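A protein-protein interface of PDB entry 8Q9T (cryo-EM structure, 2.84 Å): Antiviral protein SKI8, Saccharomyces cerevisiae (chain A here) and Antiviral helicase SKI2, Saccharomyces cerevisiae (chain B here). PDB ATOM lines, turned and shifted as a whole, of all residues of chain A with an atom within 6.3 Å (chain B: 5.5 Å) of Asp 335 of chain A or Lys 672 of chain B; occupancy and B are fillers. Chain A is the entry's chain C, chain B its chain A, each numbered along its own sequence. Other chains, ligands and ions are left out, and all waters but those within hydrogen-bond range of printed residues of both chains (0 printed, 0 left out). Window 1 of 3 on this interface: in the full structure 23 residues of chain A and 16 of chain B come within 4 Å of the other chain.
N of Lys 673 of chain B lies within hydrogen-bond range of O of Asp 334 of chain A (3.2 Å).
NH1 of Arg 676 of chain B is in hydrogen-bond range of O of Ile 336 of chain A, at 3.5 Å.
OG1 of Thr 669 of chain B is in hydrogen-bond range of OE2 of Glu 337 of chain A.
The backbone carbonyl oxygen (O) of Asp 335 of chain A sits at hydrogen-bond distance from the guanidinium group (NH2) of Arg 676 of chain B, 3.3 Å away.
NZ of Lys 672 of chain B lies within salt-bridge range of OE2 of Glu 674 of chain B, 2.7 Å away.
OD2 of Asp 1278 of chain B lies within salt-bridge range of NZ of Lys 672 of chain B (3.8 Å).
The side-chain amide nitrogen of Asn 10 of chain A sits at hydrogen-bond distance from the backbone carbonyl oxygen of Asp 335 of chain A (3.0 Å).
The side-chain amino group (NZ) of Lys 673 of chain B is in salt-bridge range of the side-chain carboxylate (OD2) of Asp 677 of chain B (3.9 Å).
OD2 of Asp 335 of chain A sits at hydrogen-bond distance from N of His 332 of chain A (3.2 Å).
The backbone carbonyl oxygen (O) of His 332 of chain A sits at hydrogen-bond distance from the guanidinium group (NH2) of Arg 389 of chain A (2.6 Å).
Among the printed residues, merely in contact across the chains: His 332 of chain A with Lys 672 of chain B (3.3 Å), Asp 334 of chain A with Arg 676 of chain B (3.8 Å), Asp 335 of chain A with Lys 672 of chain B (3.4 Å) and Ile 342 of chain A with Lys 673 of chain B (3.9 Å).
Of the printed residues of chain B, His 332 of chain A touches Lys 672 (3.3 Å).
Printed residues of chain B within 4 Å of Asp 334 of chain A: Lys 673 (3.2 Å) and Arg 676 (3.8 Å).
Asp 335 of chain A touches two residues of chain B.
Of the printed residues of chain A, Lys 672 of chain B touches His 332 (3.3 Å) and Asp 335 (3.4 Å).
The nearest printed residue of chain A that does not touch Lys 672 of chain B is Asp 334 of chain A (4.01 Å).
Of the 13 printed residues of chain A, 6 touch a printed residue of chain B.
Printed residues of chain A that touch a printed residue of chain B: His 332, Asp 334, Asp 335, Ile 336, Glu 337 and Ile 342.
Hydrophobic or aromatic side chains of chain A within 4 Å of the printed part of chain B: His 332 and Ile 342.
Of the 11 printed residues of chain B, 4 touch a printed residue of chain A.
Printed residues of chain B that touch a printed residue of chain A: Thr 669, Lys 672, Lys 673 and Arg 676.
Among the printed residues, 8 pairs touch across the chains.
Among the printed residues, no Asp or Glu carboxylate lies within 4 Å of a Lys or Arg side-chain nitrogen of the other chain.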
ATOM      1  N   ASN A  10     -15.787  -9.061 -23.788  1.00  0.00           N
ATOM      2  CA  ASN A  10     -14.567  -8.604 -24.431  1.00  0.00           C
ATOM      3  C   ASN A  10     -13.383  -9.362 -23.851  1.00  0.00           C
ATOM      4  O   ASN A  10     -13.459  -9.923 -22.757  1.00  0.00           O
ATOM      5  CB  ASN A  10     -14.395  -7.093 -24.250  1.00  0.00           C
ATOM      6  CG  ASN A  10     -13.546  -6.472 -25.323  1.00  0.00           C
ATOM      7  OD1 ASN A  10     -12.967  -7.170 -26.150  1.00  0.00           O
ATOM      8  ND2 ASN A  10     -13.482  -5.151 -25.332  1.00  0.00           N
ATOM      9  N   ASN A 330     -17.550   1.713 -34.579  1.00  0.00           N
ATOM     10  CA  ASN A 330     -16.158   2.136 -34.543  1.00  0.00           C
ATOM     11  C   ASN A 330     -15.383   1.294 -33.540  1.00  0.00           C
ATOM     12  O   ASN A 330     -15.880   0.996 -32.451  1.00  0.00           O
ATOM     13  CB  ASN A 330     -16.044   3.617 -34.175  1.00  0.00           C
ATOM     14  CG  ASN A 330     -16.661   4.526 -35.217  1.00  0.00           C
ATOM     15  OD1 ASN A 330     -16.255   4.523 -36.378  1.00  0.00           O
ATOM     16  ND2 ASN A 330     -17.649   5.310 -34.808  1.00  0.00           N
ATOM     17  N   MET A 331     -14.164   0.915 -33.911  1.00  0.00           N
ATOM     18  CA  MET A 331     -13.303   0.083 -33.081  1.00  0.00           C
ATOM     19  C   MET A 331     -12.179   0.928 -32.500  1.00  0.00           C
ATOM     20  O   MET A 331     -11.495   1.646 -33.234  1.00  0.00           O
ATOM     21  CB  MET A 331     -12.713  -1.078 -33.886  1.00  0.00           C
ATOM     22  CG  MET A 331     -13.738  -2.011 -34.502  1.00  0.00           C
ATOM     23  SD  MET A 331     -14.649  -2.961 -33.276  1.00  0.00           S
ATOM     24  CE  MET A 331     -16.328  -2.637 -33.796  1.00  0.00           C
ATOM     25  N   HIS A 332     -11.991   0.834 -31.187  1.00  0.00           N
ATOM     26  CA  HIS A 332     -10.901   1.504 -30.498  1.00  0.00           C
ATOM     27  C   HIS A 332     -10.170   0.501 -29.620  1.00  0.00           C
ATOM     28  O   HIS A 332     -10.723  -0.526 -29.221  1.00  0.00           O
ATOM     29  CB  HIS A 332     -11.399   2.675 -29.639  1.00  0.00           C
ATOM     30  CG  HIS A 332     -12.349   3.588 -30.349  1.00  0.00           C
ATOM     31  ND1 HIS A 332     -13.717   3.474 -30.234  1.00  0.00           N
ATOM     32  CD2 HIS A 332     -12.127   4.634 -31.178  1.00  0.00           C
ATOM     33  CE1 HIS A 332     -14.297   4.409 -30.964  1.00  0.00           C
ATOM     34  NE2 HIS A 332     -13.355   5.127 -31.547  1.00  0.00           N
ATOM     35  N   CYS A 333      -8.908   0.807 -29.322  1.00  0.00           N
ATOM     36  CA  CYS A 333      -8.150  -0.021 -28.394  1.00  0.00           C
ATOM     37  C   CYS A 333      -8.637   0.132 -26.961  1.00  0.00           C
ATOM     38  O   CYS A 333      -8.329  -0.720 -26.121  1.00  0.00           O
ATOM     39  CB  CYS A 333      -6.663   0.321 -28.471  1.00  0.00           C
ATOM     40  SG  CYS A 333      -6.250   1.980 -27.899  1.00  0.00           S
ATOM     41  N   ASP A 334      -9.393   1.186 -26.668  1.00  0.00           N
ATOM     42  CA  ASP A 334      -9.868   1.479 -25.324  1.00  0.00           C
ATOM     43  C   ASP A 334     -11.199   0.816 -25.004  1.00  0.00           C
ATOM     44  O   ASP A 334     -11.750   1.056 -23.928  1.00  0.00           O
ATOM     45  CB  ASP A 334      -9.991   2.992 -25.130  1.00  0.00           C
ATOM     46  CG  ASP A 334      -8.749   3.604 -24.522  1.00  0.00           C
ATOM     47  OD1 ASP A 334      -7.712   2.912 -24.465  1.00  0.00           O
ATOM     48  OD2 ASP A 334      -8.809   4.778 -24.100  1.00  0.00           O
ATOM     49  N   ASP A 335     -11.735   0.002 -25.914  1.00  0.00           N
ATOM     50  CA  ASP A 335     -12.980  -0.708 -25.654  1.00  0.00           C
ATOM     51  C   ASP A 335     -12.813  -1.855 -24.667  1.00  0.00           C
ATOM     52  O   ASP A 335     -13.821  -2.382 -24.188  1.00  0.00           O
ATOM     53  CB  ASP A 335     -13.555  -1.249 -26.962  1.00  0.00           C
ATOM     54  CG  ASP A 335     -13.851  -0.157 -27.967  1.00  0.00           C
ATOM     55  OD1 ASP A 335     -13.888   1.024 -27.567  1.00  0.00           O
ATOM     56  OD2 ASP A 335     -14.052  -0.479 -29.155  1.00  0.00           O
ATOM     57  N   ILE A 336     -11.579  -2.252 -24.358  1.00  0.00           N
ATOM     58  CA  ILE A 336     -11.347  -3.402 -23.494  1.00  0.00           C
ATOM     59  C   ILE A 336     -11.780  -3.072 -22.075  1.00  0.00           C
ATOM     60  O   ILE A 336     -11.469  -1.997 -21.547  1.00  0.00           O
ATOM     61  CB  ILE A 336      -9.873  -3.824 -23.549  1.00  0.00           C
ATOM     62  CG1 ILE A 336      -9.409  -3.931 -25.001  1.00  0.00           C
ATOM     63  CG2 ILE A 336      -9.666  -5.142 -22.829  1.00  0.00           C
ATOM     64  CD1 ILE A 336     -10.126  -4.996 -25.790  1.00  0.00           C
ATOM     65  N   GLU A 337     -12.504  -4.002 -21.447  1.00  0.00           N
ATOM     66  CA  GLU A 337     -13.021  -3.767 -20.104  1.00  0.00           C
ATOM     67  C   GLU A 337     -11.907  -3.754 -19.065  1.00  0.00           C
ATOM     68  O   GLU A 337     -11.905  -2.912 -18.161  1.00  0.00           O
ATOM     69  CB  GLU A 337     -14.062  -4.827 -19.755  1.00  0.00           C
ATOM     70  CG  GLU A 337     -15.398  -4.634 -20.437  1.00  0.00           C
ATOM     71  CD  GLU A 337     -16.344  -5.791 -20.188  1.00  0.00           C
ATOM     72  OE1 GLU A 337     -16.293  -6.776 -20.954  1.00  0.00           O
ATOM     73  OE2 GLU A 337     -17.136  -5.718 -19.224  1.00  0.00           O
ATOM     74  N   ILE A 338     -10.959  -4.682 -19.167  1.00  0.00           N
ATOM     75  CA  ILE A 338      -9.833  -4.749 -18.244  1.00  0.00           C
ATOM     76  C   ILE A 338      -8.733  -3.834 -18.765  1.00  0.00           C
ATOM     77  O   ILE A 338      -8.292  -3.970 -19.911  1.00  0.00           O
ATOM     78  CB  ILE A 338      -9.326  -6.190 -18.084  1.00  0.00           C
ATOM     79  CG1 ILE A 338     -10.363  -7.040 -17.353  1.00  0.00           C
ATOM     80  CG2 ILE A 338      -8.007  -6.212 -17.339  1.00  0.00           C
ATOM     81  CD1 ILE A 338      -9.991  -8.497 -17.249  1.00  0.00           C
ATOM     82  N   ILE A 342      -5.156  -3.617 -22.459  1.00  0.00           N
ATOM     83  CA  ILE A 342      -5.269  -2.644 -23.540  1.00  0.00           C
ATOM     84  C   ILE A 342      -3.913  -2.514 -24.222  1.00  0.00           C
ATOM     85  O   ILE A 342      -2.913  -2.182 -23.577  1.00  0.00           O
ATOM     86  CB  ILE A 342      -5.757  -1.288 -23.013  1.00  0.00           C
ATOM     87  CG1 ILE A 342      -7.200  -1.400 -22.520  1.00  0.00           C
ATOM     88  CG2 ILE A 342      -5.636  -0.225 -24.089  1.00  0.00           C
ATOM     89  CD1 ILE A 342      -7.863  -0.073 -22.256  1.00  0.00           C
ATOM     90  N   ARG A 389     -14.162  -9.527 -29.601  1.00  0.00           N
ATOM     91  CA  ARG A 389     -15.260  -8.732 -29.072  1.00  0.00           C
ATOM     92  C   ARG A 389     -16.599  -9.328 -29.481  1.00  0.00           C
ATOM     93  O   ARG A 389     -16.739  -9.894 -30.567  1.00  0.00           O
ATOM     94  CB  ARG A 389     -15.167  -7.281 -29.559  1.00  0.00           C
ATOM     95  CG  ARG A 389     -13.756  -6.728 -29.542  1.00  0.00           C
ATOM     96  CD  ARG A 389     -13.707  -5.282 -29.962  1.00  0.00           C
ATOM     97  NE  ARG A 389     -12.366  -4.732 -29.820  1.00  0.00           N
ATOM     98  CZ  ARG A 389     -12.084  -3.437 -29.831  1.00  0.00           C
ATOM     99  NH1 ARG A 389     -13.030  -2.526 -29.976  1.00  0.00           N
ATOM    100  NH2 ARG A 389     -10.821  -3.047 -29.692  1.00  0.00           N
ATOM    101  N   PHE A 391     -21.015  -8.695 -29.473  1.00  0.00           N
ATOM    102  CA  PHE A 391     -22.056  -7.679 -29.509  1.00  0.00           C
ATOM    103  C   PHE A 391     -23.429  -8.334 -29.468  1.00  0.00           C
ATOM    104  O   PHE A 391     -23.587  -9.518 -29.769  1.00  0.00           O
ATOM    105  CB  PHE A 391     -21.936  -6.794 -30.758  1.00  0.00           C
ATOM    106  CG  PHE A 391     -20.710  -5.931 -30.773  1.00  0.00           C
ATOM    107  CD1 PHE A 391     -20.737  -4.660 -30.232  1.00  0.00           C
ATOM    108  CD2 PHE A 391     -19.531  -6.388 -31.332  1.00  0.00           C
ATOM    109  CE1 PHE A 391     -19.613  -3.869 -30.244  1.00  0.00           C
ATOM    110  CE2 PHE A 391     -18.404  -5.598 -31.345  1.00  0.00           C
ATOM    111  CZ  PHE A 391     -18.445  -4.338 -30.801  1.00  0.00           C
ATOM    112  N   THR B 669     -20.317  -0.926 -19.489  1.00  0.00           N
ATOM    113  CA  THR B 669     -19.457  -1.717 -20.366  1.00  0.00           C
ATOM    114  C   THR B 669     -19.494  -1.207 -21.802  1.00  0.00           C
ATOM    115  O   THR B 669     -18.491  -1.291 -22.519  1.00  0.00           O
ATOM    116  CB  THR B 669     -19.875  -3.189 -20.306  1.00  0.00           C
ATOM    117  OG1 THR B 669     -19.571  -3.719 -19.011  1.00  0.00           O
ATOM    118  CG2 THR B 669     -19.156  -4.013 -21.358  1.00  0.00           C
ATOM    119  N   ARG B 670     -20.626  -0.650 -22.231  1.00  0.00           N
ATOM    120  CA  ARG B 670     -20.798  -0.213 -23.609  1.00  0.00           C
ATOM    121  C   ARG B 670     -19.970   1.017 -23.960  1.00  0.00           C
ATOM    122  O   ARG B 670     -19.904   1.376 -25.140  1.00  0.00           O
ATOM    123  CB  ARG B 670     -22.276   0.072 -23.877  1.00  0.00           C
ATOM    124  CG  ARG B 670     -22.913   1.012 -22.865  1.00  0.00           C
ATOM    125  CD  ARG B 670     -24.425   1.011 -22.974  1.00  0.00           C
ATOM    126  NE  ARG B 670     -25.023  -0.102 -22.247  1.00  0.00           N
ATOM    127  CZ  ARG B 670     -26.257  -0.545 -22.439  1.00  0.00           C
ATOM    128  NH1 ARG B 670     -27.059   0.010 -23.328  1.00  0.00           N
ATOM    129  NH2 ARG B 670     -26.695  -1.573 -21.720  1.00  0.00           N
ATOM    130  N   LEU B 671     -19.346   1.668 -22.985  1.00  0.00           N
ATOM    131  CA  LEU B 671     -18.601   2.897 -23.204  1.00  0.00           C
ATOM    132  C   LEU B 671     -17.105   2.624 -23.331  1.00  0.00           C
ATOM    133  O   LEU B 671     -16.594   1.593 -22.890  1.00  0.00           O
ATOM    134  CB  LEU B 671     -18.848   3.886 -22.063  1.00  0.00           C
ATOM    135  CG  LEU B 671     -20.296   4.249 -21.743  1.00  0.00           C
ATOM    136  CD1 LEU B 671     -20.341   5.213 -20.577  1.00  0.00           C
ATOM    137  CD2 LEU B 671     -20.976   4.848 -22.957  1.00  0.00           C
ATOM    138  N   LYS B 672     -16.405   3.577 -23.943  1.00  0.00           N
ATOM    139  CA  LYS B 672     -14.953   3.536 -24.014  1.00  0.00           C
ATOM    140  C   LYS B 672     -14.346   3.826 -22.644  1.00  0.00           C
ATOM    141  O   LYS B 672     -15.024   4.267 -21.714  1.00  0.00           O
ATOM    142  CB  LYS B 672     -14.431   4.551 -25.023  1.00  0.00           C
ATOM    143  CG  LYS B 672     -14.528   4.122 -26.462  1.00  0.00           C
ATOM    144  CD  LYS B 672     -13.634   4.992 -27.319  1.00  0.00           C
ATOM    145  CE  LYS B 672     -14.024   6.450 -27.205  1.00  0.00           C
ATOM    146  NZ  LYS B 672     -13.214   7.300 -28.115  1.00  0.00           N
ATOM    147  N   LYS B 673     -13.038   3.584 -22.532  1.00  0.00           N
ATOM    148  CA  LYS B 673     -12.358   3.808 -21.260  1.00  0.00           C
ATOM    149  C   LYS B 673     -12.366   5.281 -20.878  1.00  0.00           C
ATOM    150  O   LYS B 673     -12.577   5.625 -19.710  1.00  0.00           O
ATOM    151  CB  LYS B 673     -10.927   3.282 -21.321  1.00  0.00           C
ATOM    152  CG  LYS B 673     -10.145   3.556 -20.053  1.00  0.00           C
ATOM    153  CD  LYS B 673      -8.712   3.087 -20.156  1.00  0.00           C
ATOM    154  CE  LYS B 673      -7.869   3.715 -19.061  1.00  0.00           C
ATOM    155  NZ  LYS B 673      -8.370   3.351 -17.708  1.00  0.00           N
ATOM    156  N   GLU B 674     -12.132   6.170 -21.845  1.00  0.00           N
ATOM    157  CA  GLU B 674     -12.177   7.596 -21.547  1.00  0.00           C
ATOM    158  C   GLU B 674     -13.592   8.079 -21.267  1.00  0.00           C
ATOM    159  O   GLU B 674     -13.762   9.103 -20.598  1.00  0.00           O
ATOM    160  CB  GLU B 674     -11.562   8.399 -22.693  1.00  0.00           C
ATOM    161  CG  GLU B 674     -12.179   8.135 -24.049  1.00  0.00           C
ATOM    162  CD  GLU B 674     -11.395   8.786 -25.171  1.00  0.00           C
ATOM    163  OE1 GLU B 674     -10.312   9.340 -24.896  1.00  0.00           O
ATOM    164  OE2 GLU B 674     -11.862   8.746 -26.329  1.00  0.00           O
ATOM    165  N   ASP B 675     -14.607   7.371 -21.764  1.00  0.00           N
ATOM    166  CA  ASP B 675     -15.984   7.712 -21.431  1.00  0.00           C
ATOM    167  C   ASP B 675     -16.337   7.273 -20.016  1.00  0.00           C
ATOM    168  O   ASP B 675     -17.053   7.985 -19.308  1.00  0.00           O
ATOM    169  CB  ASP B 675     -16.944   7.080 -22.436  1.00  0.00           C
ATOM    170  CG  ASP B 675     -16.956   7.801 -23.767  1.00  0.00           C
ATOM    171  OD1 ASP B 675     -16.487   8.954 -23.825  1.00  0.00           O
ATOM    172  OD2 ASP B 675     -17.432   7.211 -24.757  1.00  0.00           O
ATOM    173  N   ARG B 676     -15.842   6.109 -19.588  1.00  0.00           N
ATOM    174  CA  ARG B 676     -16.113   5.626 -18.240  1.00  0.00           C
ATOM    175  C   ARG B 676     -15.440   6.475 -17.172  1.00  0.00           C
ATOM    176  O   ARG B 676     -15.814   6.382 -15.999  1.00  0.00           O
ATOM    177  CB  ARG B 676     -15.649   4.179 -18.087  1.00  0.00           C
ATOM    178  CG  ARG B 676     -16.299   3.191 -19.029  1.00  0.00           C
ATOM    179  CD  ARG B 676     -15.604   1.843 -18.946  1.00  0.00           C
ATOM    180  NE  ARG B 676     -15.663   1.115 -20.207  1.00  0.00           N
ATOM    181  CZ  ARG B 676     -14.630   0.503 -20.768  1.00  0.00           C
ATOM    182  NH1 ARG B 676     -13.431   0.516 -20.210  1.00  0.00           N
ATOM    183  NH2 ARG B 676     -14.803  -0.136 -21.921  1.00  0.00           N
ATOM    184  N   ASP B 677     -14.458   7.290 -17.546  1.00  0.00           N
ATOM    185  CA  ASP B 677     -13.685   8.078 -16.599  1.00  0.00           C
ATOM    186  C   ASP B 677     -14.172   9.517 -16.494  1.00  0.00           C
ATOM    187  O   ASP B 677     -13.483  10.350 -15.898  1.00  0.00           O
ATOM    188  CB  ASP B 677     -12.207   8.054 -16.987  1.00  0.00           C
ATOM    189  CG  ASP B 677     -11.513   6.777 -16.555  1.00  0.00           C
ATOM    190  OD1 ASP B 677     -12.149   5.957 -15.862  1.00  0.00           O
ATOM    191  OD2 ASP B 677     -10.332   6.590 -16.916  1.00  0.00           O
ATOM    192  N   ARG B1277     -21.733   9.067 -32.768  1.00  0.00           N
ATOM    193  CA  ARG B1277     -20.754   8.175 -32.161  1.00  0.00           C
ATOM    194  C   ARG B1277     -20.718   8.402 -30.657  1.00  0.00           C
ATOM    195  O   ARG B1277     -21.245   9.393 -30.147  1.00  0.00           O
ATOM    196  CB  ARG B1277     -19.361   8.400 -32.752  1.00  0.00           C
ATOM    197  CG  ARG B1277     -18.951   9.858 -32.771  1.00  0.00           C
ATOM    198  CD  ARG B1277     -17.471  10.030 -33.024  1.00  0.00           C
ATOM    199  NE  ARG B1277     -17.038  11.396 -32.760  1.00  0.00           N
ATOM    200  CZ  ARG B1277     -16.245  11.747 -31.756  1.00  0.00           C
ATOM    201  NH1 ARG B1277     -15.780  10.856 -30.901  1.00  0.00           N
ATOM    202  NH2 ARG B1277     -15.915  13.026 -31.608  1.00  0.00           N
ATOM    203  N   ASP B1278     -20.094   7.457 -29.962  1.00  0.00           N
ATOM    204  CA  ASP B1278     -19.637   7.587 -28.570  1.00  0.00           C
ATOM    205  C   ASP B1278     -20.829   7.767 -27.626  1.00  0.00           C
ATOM    206  O   ASP B1278     -21.946   7.324 -27.923  1.00  0.00           O
ATOM    207  CB  ASP B1278     -18.600   8.688 -28.485  1.00  0.00           C
ATOM    208  CG  ASP B1278     -17.289   8.299 -29.134  1.00  0.00           C
ATOM    209  OD1 ASP B1278     -17.192   7.164 -29.642  1.00  0.00           O
ATOM    210  OD2 ASP B1278     -16.355   9.127 -29.137  1.00  0.00           O
